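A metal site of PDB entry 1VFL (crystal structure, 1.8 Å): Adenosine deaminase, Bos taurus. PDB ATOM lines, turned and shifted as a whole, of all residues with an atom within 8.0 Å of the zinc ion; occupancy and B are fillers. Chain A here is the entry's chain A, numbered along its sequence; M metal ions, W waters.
The side-chain carboxylate of Asp 294 sits at hydrogen-bond distance from the side-chain hydroxyl of Ser 264, 3.0 Å away.
O of Glu 259 is in hydrogen-bond range of N of His 237 (2.8 Å).
N of His 213 lies within hydrogen-bond range of O of Leu 181, 2.9 Å away.
A ring nitrogen (NE2) of His 237 sits close to the side-chain carboxylate (OE2) of Glu 216 (3.3 Å).
ND1 of His 213 lies close to OD1 of Asp 180.
The backbone NH (N) of His 14 lies within hydrogen-bond range of the side-chain amide oxygen (OD1) of Asn 292 (2.9 Å).
A ring nitrogen (ND1) of His 14 is in hydrogen-bond range of the side-chain carboxylate (OE1) of Glu 259 (2.7 Å).
The zinc ion is bound by a ring nitrogen (NE2) of His 16 (2.0 Å), water W1 (2.1 Å), a ring nitrogen (NE2) of His 14 (2.1 Å), a ring nitrogen (NE2) of His 213 (2.2 Å) and the side-chain carboxylate (OD1) of Asp 294 (2.4 Å).
Residues that only touch the zinc ion: His 237.
The nearest printed residue that does not touch the zinc ion is Asp 295 (4.8 Å).
Water W1 lies within hydrogen-bond range of OD2 of Asp 294 and NE2 of His 237.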
ATOM      1  N   HIS A  14      14.779  -7.780   1.232  1.00  0.00           N
ATOM      2  CA  HIS A  14      13.373  -7.932   1.544  1.00  0.00           C
ATOM      3  C   HIS A  14      12.969  -9.385   1.800  1.00  0.00           C
ATOM      4  O   HIS A  14      12.693 -10.142   0.873  1.00  0.00           O
ATOM      5  CB  HIS A  14      12.544  -7.325   0.418  1.00  0.00           C
ATOM      6  CG  HIS A  14      11.089  -7.173   0.731  1.00  0.00           C
ATOM      7  ND1 HIS A  14      10.402  -5.992   0.529  1.00  0.00           N
ATOM      8  CD2 HIS A  14      10.160  -8.068   1.161  1.00  0.00           C
ATOM      9  CE1 HIS A  14       9.124  -6.164   0.806  1.00  0.00           C
ATOM     10  NE2 HIS A  14       8.951  -7.421   1.197  1.00  0.00           N
ATOM     11  N   VAL A  15      12.955  -9.762   3.076  1.00  0.00           N
ATOM     12  CA  VAL A  15      12.594 -11.110   3.498  1.00  0.00           C
ATOM     13  C   VAL A  15      12.098 -11.000   4.940  1.00  0.00           C
ATOM     14  O   VAL A  15      12.747 -10.377   5.784  1.00  0.00           O
ATOM     15  CB  VAL A  15      13.797 -12.098   3.385  1.00  0.00           C
ATOM     16  CG1 VAL A  15      14.994 -11.564   4.183  1.00  0.00           C
ATOM     17  CG2 VAL A  15      13.380 -13.478   3.903  1.00  0.00           C
ATOM     18  N   HIS A  16      10.945 -11.600   5.197  1.00  0.00           N
ATOM     19  CA  HIS A  16      10.295 -11.561   6.515  1.00  0.00           C
ATOM     20  C   HIS A  16      10.690 -12.754   7.393  1.00  0.00           C
ATOM     21  O   HIS A  16      10.517 -13.904   7.007  1.00  0.00           O
ATOM     22  CB  HIS A  16       8.767 -11.565   6.335  1.00  0.00           C
ATOM     23  CG  HIS A  16       8.232 -10.401   5.541  1.00  0.00           C
ATOM     24  ND1 HIS A  16       7.599  -9.337   6.128  1.00  0.00           N
ATOM     25  CD2 HIS A  16       8.219 -10.159   4.205  1.00  0.00           C
ATOM     26  CE1 HIS A  16       7.204  -8.489   5.205  1.00  0.00           C
ATOM     27  NE2 HIS A  16       7.570  -8.962   4.021  1.00  0.00           N
ATOM     28  N   PHE A  60      -4.381 -16.125   2.190  1.00  0.00           N
ATOM     29  CA  PHE A  60      -2.961 -15.857   2.356  1.00  0.00           C
ATOM     30  C   PHE A  60      -2.607 -15.570   3.816  1.00  0.00           C
ATOM     31  O   PHE A  60      -1.712 -16.206   4.381  1.00  0.00           O
ATOM     32  CB  PHE A  60      -2.538 -14.662   1.514  1.00  0.00           C
ATOM     33  CG  PHE A  60      -1.066 -14.378   1.577  1.00  0.00           C
ATOM     34  CD1 PHE A  60      -0.168 -15.227   0.971  1.00  0.00           C
ATOM     35  CD2 PHE A  60      -0.595 -13.283   2.272  1.00  0.00           C
ATOM     36  CE1 PHE A  60       1.197 -14.995   1.060  1.00  0.00           C
ATOM     37  CE2 PHE A  60       0.764 -13.042   2.370  1.00  0.00           C
ATOM     38  CZ  PHE A  60       1.654 -13.896   1.764  1.00  0.00           C
ATOM     39  N   ARG A 100      13.310  -8.520   8.120  1.00  0.00           N
ATOM     40  CA  ARG A 100      12.283  -7.723   8.763  1.00  0.00           C
ATOM     41  C   ARG A 100      11.189  -8.553   9.423  1.00  0.00           C
ATOM     42  O   ARG A 100      10.995  -9.721   9.080  1.00  0.00           O
ATOM     43  CB  ARG A 100      11.653  -6.778   7.749  1.00  0.00           C
ATOM     44  CG  ARG A 100      10.844  -7.497   6.664  1.00  0.00           C
ATOM     45  CD  ARG A 100      10.349  -6.505   5.624  1.00  0.00           C
ATOM     46  NE  ARG A 100      11.453  -6.037   4.780  1.00  0.00           N
ATOM     47  CZ  ARG A 100      11.327  -5.089   3.856  1.00  0.00           C
ATOM     48  NH1 ARG A 100      12.385  -4.738   3.130  1.00  0.00           N
ATOM     49  NH2 ARG A 100      10.167  -4.472   3.674  1.00  0.00           N
ATOM     50  N   CYS A 152       8.836  -3.862  11.472  1.00  0.00           N
ATOM     51  CA  CYS A 152       7.644  -3.571  10.704  1.00  0.00           C
ATOM     52  C   CYS A 152       6.441  -2.995  11.420  1.00  0.00           C
ATOM     53  O   CYS A 152       5.994  -3.527  12.439  1.00  0.00           O
ATOM     54  CB  CYS A 152       7.142  -4.842  10.008  1.00  0.00           C
ATOM     55  SG  CYS A 152       8.232  -5.583   8.820  1.00  0.00           S
ATOM     56  N   ASP A 180       9.824  -0.372   8.672  1.00  0.00           N
ATOM     57  CA  ASP A 180       9.059  -0.779   7.488  1.00  0.00           C
ATOM     58  C   ASP A 180       7.566  -0.609   7.766  1.00  0.00           C
ATOM     59  O   ASP A 180       7.155  -0.352   8.903  1.00  0.00           O
ATOM     60  CB  ASP A 180       9.356  -2.257   7.143  1.00  0.00           C
ATOM     61  CG  ASP A 180       8.608  -2.738   5.889  1.00  0.00           C
ATOM     62  OD1 ASP A 180       8.405  -3.961   5.747  1.00  0.00           O
ATOM     63  OD2 ASP A 180       8.241  -1.907   5.040  1.00  0.00           O
ATOM     64  N   LEU A 181       6.754  -0.734   6.718  1.00  0.00           N
ATOM     65  CA  LEU A 181       5.306  -0.641   6.807  1.00  0.00           C
ATOM     66  C   LEU A 181       4.819  -1.786   5.949  1.00  0.00           C
ATOM     67  O   LEU A 181       5.007  -1.792   4.727  1.00  0.00           O
ATOM     68  CB  LEU A 181       4.819   0.697   6.209  1.00  0.00           C
ATOM     69  CG  LEU A 181       3.533   1.345   6.749  1.00  0.00           C
ATOM     70  CD1 LEU A 181       2.843   2.088   5.614  1.00  0.00           C
ATOM     71  CD2 LEU A 181       2.594   0.318   7.352  1.00  0.00           C
ATOM     72  N   ALA A 182       4.191  -2.778   6.572  1.00  0.00           N
ATOM     73  CA  ALA A 182       3.692  -3.943   5.858  1.00  0.00           C
ATOM     74  C   ALA A 182       2.226  -4.205   6.176  1.00  0.00           C
ATOM     75  O   ALA A 182       1.644  -3.512   6.996  1.00  0.00           O
ATOM     76  CB  ALA A 182       4.522  -5.162   6.211  1.00  0.00           C
ATOM     77  N   GLY A 183       1.656  -5.210   5.537  1.00  0.00           N
ATOM     78  CA  GLY A 183       0.260  -5.538   5.766  1.00  0.00           C
ATOM     79  C   GLY A 183      -0.591  -5.325   4.530  1.00  0.00           C
ATOM     80  O   GLY A 183      -0.074  -5.257   3.415  1.00  0.00           O
ATOM     81  N   HIS A 213       6.166  -1.075   2.132  1.00  0.00           N
ATOM     82  CA  HIS A 213       5.570  -1.987   1.153  1.00  0.00           C
ATOM     83  C   HIS A 213       4.536  -1.136   0.399  1.00  0.00           C
ATOM     84  O   HIS A 213       3.560  -0.673   1.006  1.00  0.00           O
ATOM     85  CB  HIS A 213       4.815  -3.148   1.821  1.00  0.00           C
ATOM     86  CG  HIS A 213       5.665  -4.290   2.274  1.00  0.00           C
ATOM     87  ND1 HIS A 213       6.499  -4.214   3.371  1.00  0.00           N
ATOM     88  CD2 HIS A 213       5.717  -5.578   1.853  1.00  0.00           C
ATOM     89  CE1 HIS A 213       7.016  -5.401   3.612  1.00  0.00           C
ATOM     90  NE2 HIS A 213       6.561  -6.246   2.706  1.00  0.00           N
ATOM     91  N   GLU A 216       2.592  -3.240  -4.496  1.00  0.00           N
ATOM     92  CA  GLU A 216       2.642  -4.684  -4.699  1.00  0.00           C
ATOM     93  C   GLU A 216       1.307  -5.072  -5.320  1.00  0.00           C
ATOM     94  O   GLU A 216       1.262  -5.703  -6.375  1.00  0.00           O
ATOM     95  CB  GLU A 216       2.825  -5.404  -3.355  1.00  0.00           C
ATOM     96  CG  GLU A 216       3.008  -6.916  -3.473  1.00  0.00           C
ATOM     97  CD  GLU A 216       3.108  -7.614  -2.113  1.00  0.00           C
ATOM     98  OE1 GLU A 216       2.976  -6.930  -1.071  1.00  0.00           O
ATOM     99  OE2 GLU A 216       3.315  -8.847  -2.094  1.00  0.00           O
ATOM    100  N   GLY A 236       9.077  -1.545  -1.060  1.00  0.00           N
ATOM    101  CA  GLY A 236       8.920  -2.993  -1.074  1.00  0.00           C
ATOM    102  C   GLY A 236       8.025  -3.272  -2.282  1.00  0.00           C
ATOM    103  O   GLY A 236       6.916  -2.758  -2.345  1.00  0.00           O
ATOM    104  N   HIS A 237       8.530  -4.048  -3.232  1.00  0.00           N
ATOM    105  CA  HIS A 237       7.826  -4.391  -4.476  1.00  0.00           C
ATOM    106  C   HIS A 237       7.738  -3.166  -5.404  1.00  0.00           C
ATOM    107  O   HIS A 237       8.564  -2.997  -6.317  1.00  0.00           O
ATOM    108  CB  HIS A 237       6.413  -4.910  -4.177  1.00  0.00           C
ATOM    109  CG  HIS A 237       6.390  -6.067  -3.211  1.00  0.00           C
ATOM    110  ND1 HIS A 237       6.791  -7.336  -3.568  1.00  0.00           N
ATOM    111  CD2 HIS A 237       6.047  -6.124  -1.912  1.00  0.00           C
ATOM    112  CE1 HIS A 237       6.713  -8.129  -2.510  1.00  0.00           C
ATOM    113  NE2 HIS A 237       6.255  -7.418  -1.488  1.00  0.00           N
ATOM    114  N   GLU A 259      12.556  -3.044  -4.046  1.00  0.00           N
ATOM    115  CA  GLU A 259      12.847  -4.358  -3.486  1.00  0.00           C
ATOM    116  C   GLU A 259      11.932  -5.369  -4.202  1.00  0.00           C
ATOM    117  O   GLU A 259      10.773  -5.568  -3.827  1.00  0.00           O
ATOM    118  CB  GLU A 259      12.555  -4.358  -1.982  1.00  0.00           C
ATOM    119  CG  GLU A 259      13.362  -3.299  -1.215  1.00  0.00           C
ATOM    120  CD  GLU A 259      12.826  -3.056   0.174  1.00  0.00           C
ATOM    121  OE1 GLU A 259      11.795  -3.667   0.537  1.00  0.00           O
ATOM    122  OE2 GLU A 259      13.431  -2.229   0.904  1.00  0.00           O
ATOM    123  N   CYS A 261      10.532  -9.002  -5.641  1.00  0.00           N
ATOM    124  CA  CYS A 261      10.373 -10.389  -5.219  1.00  0.00           C
ATOM    125  C   CYS A 261       9.601 -11.079  -6.348  1.00  0.00           C
ATOM    126  O   CYS A 261       8.390 -11.199  -6.291  1.00  0.00           O
ATOM    127  CB  CYS A 261       9.555 -10.426  -3.922  1.00  0.00           C
ATOM    128  SG  CYS A 261      10.127  -9.281  -2.616  1.00  0.00           S
ATOM    129  N   SER A 264       7.594 -14.488  -5.546  1.00  0.00           N
ATOM    130  CA  SER A 264       6.491 -14.054  -4.704  1.00  0.00           C
ATOM    131  C   SER A 264       5.382 -13.399  -5.549  1.00  0.00           C
ATOM    132  O   SER A 264       4.205 -13.795  -5.478  1.00  0.00           O
ATOM    133  CB  SER A 264       7.002 -13.054  -3.660  1.00  0.00           C
ATOM    134  OG  SER A 264       5.937 -12.336  -3.055  1.00  0.00           O
ATOM    135  N   ASN A 292      14.661 -10.582  -4.206  1.00  0.00           N
ATOM    136  CA  ASN A 292      14.364 -11.042  -2.841  1.00  0.00           C
ATOM    137  C   ASN A 292      13.318 -12.157  -2.763  1.00  0.00           C
ATOM    138  O   ASN A 292      12.428 -12.226  -3.609  1.00  0.00           O
ATOM    139  CB  ASN A 292      13.838  -9.837  -2.041  1.00  0.00           C
ATOM    140  CG  ASN A 292      14.742  -8.616  -2.159  1.00  0.00           C
ATOM    141  OD1 ASN A 292      15.702  -8.483  -1.413  1.00  0.00           O
ATOM    142  ND2 ASN A 292      14.429  -7.732  -3.107  1.00  0.00           N
ATOM    143  N   THR A 293      13.411 -12.999  -1.725  1.00  0.00           N
ATOM    144  CA  THR A 293      12.468 -14.108  -1.514  1.00  0.00           C
ATOM    145  C   THR A 293      11.141 -13.720  -0.862  1.00  0.00           C
ATOM    146  O   THR A 293      10.125 -14.375  -1.090  1.00  0.00           O
ATOM    147  CB  THR A 293      13.067 -15.228  -0.624  1.00  0.00           C
ATOM    148  OG1 THR A 293      13.435 -14.688   0.644  1.00  0.00           O
ATOM    149  CG2 THR A 293      14.270 -15.857  -1.301  1.00  0.00           C
ATOM    150  N   ASP A 294      11.154 -12.688  -0.014  1.00  0.00           N
ATOM    151  CA  ASP A 294       9.953 -12.210   0.687  1.00  0.00           C
ATOM    152  C   ASP A 294       9.525 -13.152   1.833  1.00  0.00           C
ATOM    153  O   ASP A 294       9.766 -12.855   3.005  1.00  0.00           O
ATOM    154  CB  ASP A 294       8.794 -12.023  -0.317  1.00  0.00           C
ATOM    155  CG  ASP A 294       7.735 -11.043   0.185  1.00  0.00           C
ATOM    156  OD1 ASP A 294       7.958 -10.395   1.230  1.00  0.00           O
ATOM    157  OD2 ASP A 294       6.687 -10.895  -0.487  1.00  0.00           O
ATOM    158  N   ASP A 295       8.886 -14.273   1.474  1.00  0.00           N
ATOM    159  CA  ASP A 295       8.428 -15.261   2.465  1.00  0.00           C
ATOM    160  C   ASP A 295       8.709 -16.677   1.978  1.00  0.00           C
ATOM    161  O   ASP A 295       7.787 -17.408   1.592  1.00  0.00           O
ATOM    162  CB  ASP A 295       6.916 -15.123   2.698  1.00  0.00           C
ATOM    163  CG  ASP A 295       6.540 -13.799   3.349  1.00  0.00           C
ATOM    164  OD1 ASP A 295       6.663 -13.664   4.576  1.00  0.00           O
ATOM    165  OD2 ASP A 295       6.129 -12.882   2.607  1.00  0.00           O
ATOM    166  N   PHE A 299       6.188 -19.399   0.179  1.00  0.00           N
ATOM    167  CA  PHE A 299       6.371 -19.611  -1.242  1.00  0.00           C
ATOM    168  C   PHE A 299       7.171 -20.873  -1.582  1.00  0.00           C
ATOM    169  O   PHE A 299       7.441 -21.153  -2.747  1.00  0.00           O
ATOM    170  CB  PHE A 299       7.031 -18.368  -1.855  1.00  0.00           C
ATOM    171  CG  PHE A 299       6.271 -17.104  -1.585  1.00  0.00           C
ATOM    172  CD1 PHE A 299       4.929 -16.991  -1.922  1.00  0.00           C
ATOM    173  CD2 PHE A 299       6.890 -16.014  -0.979  1.00  0.00           C
ATOM    174  CE1 PHE A 299       4.217 -15.841  -1.654  1.00  0.00           C
ATOM    175  CE2 PHE A 299       6.187 -14.858  -0.711  1.00  0.00           C
ATOM    176  CZ  PHE A 299       4.847 -14.769  -1.055  1.00  0.00           C
HETATM  177 ZN    ZN M   1       7.287  -8.264   2.162  1.00  0.00          ZN
HETATM  178  O   HOH W   1       5.642  -8.725   0.949  1.00  0.00           O
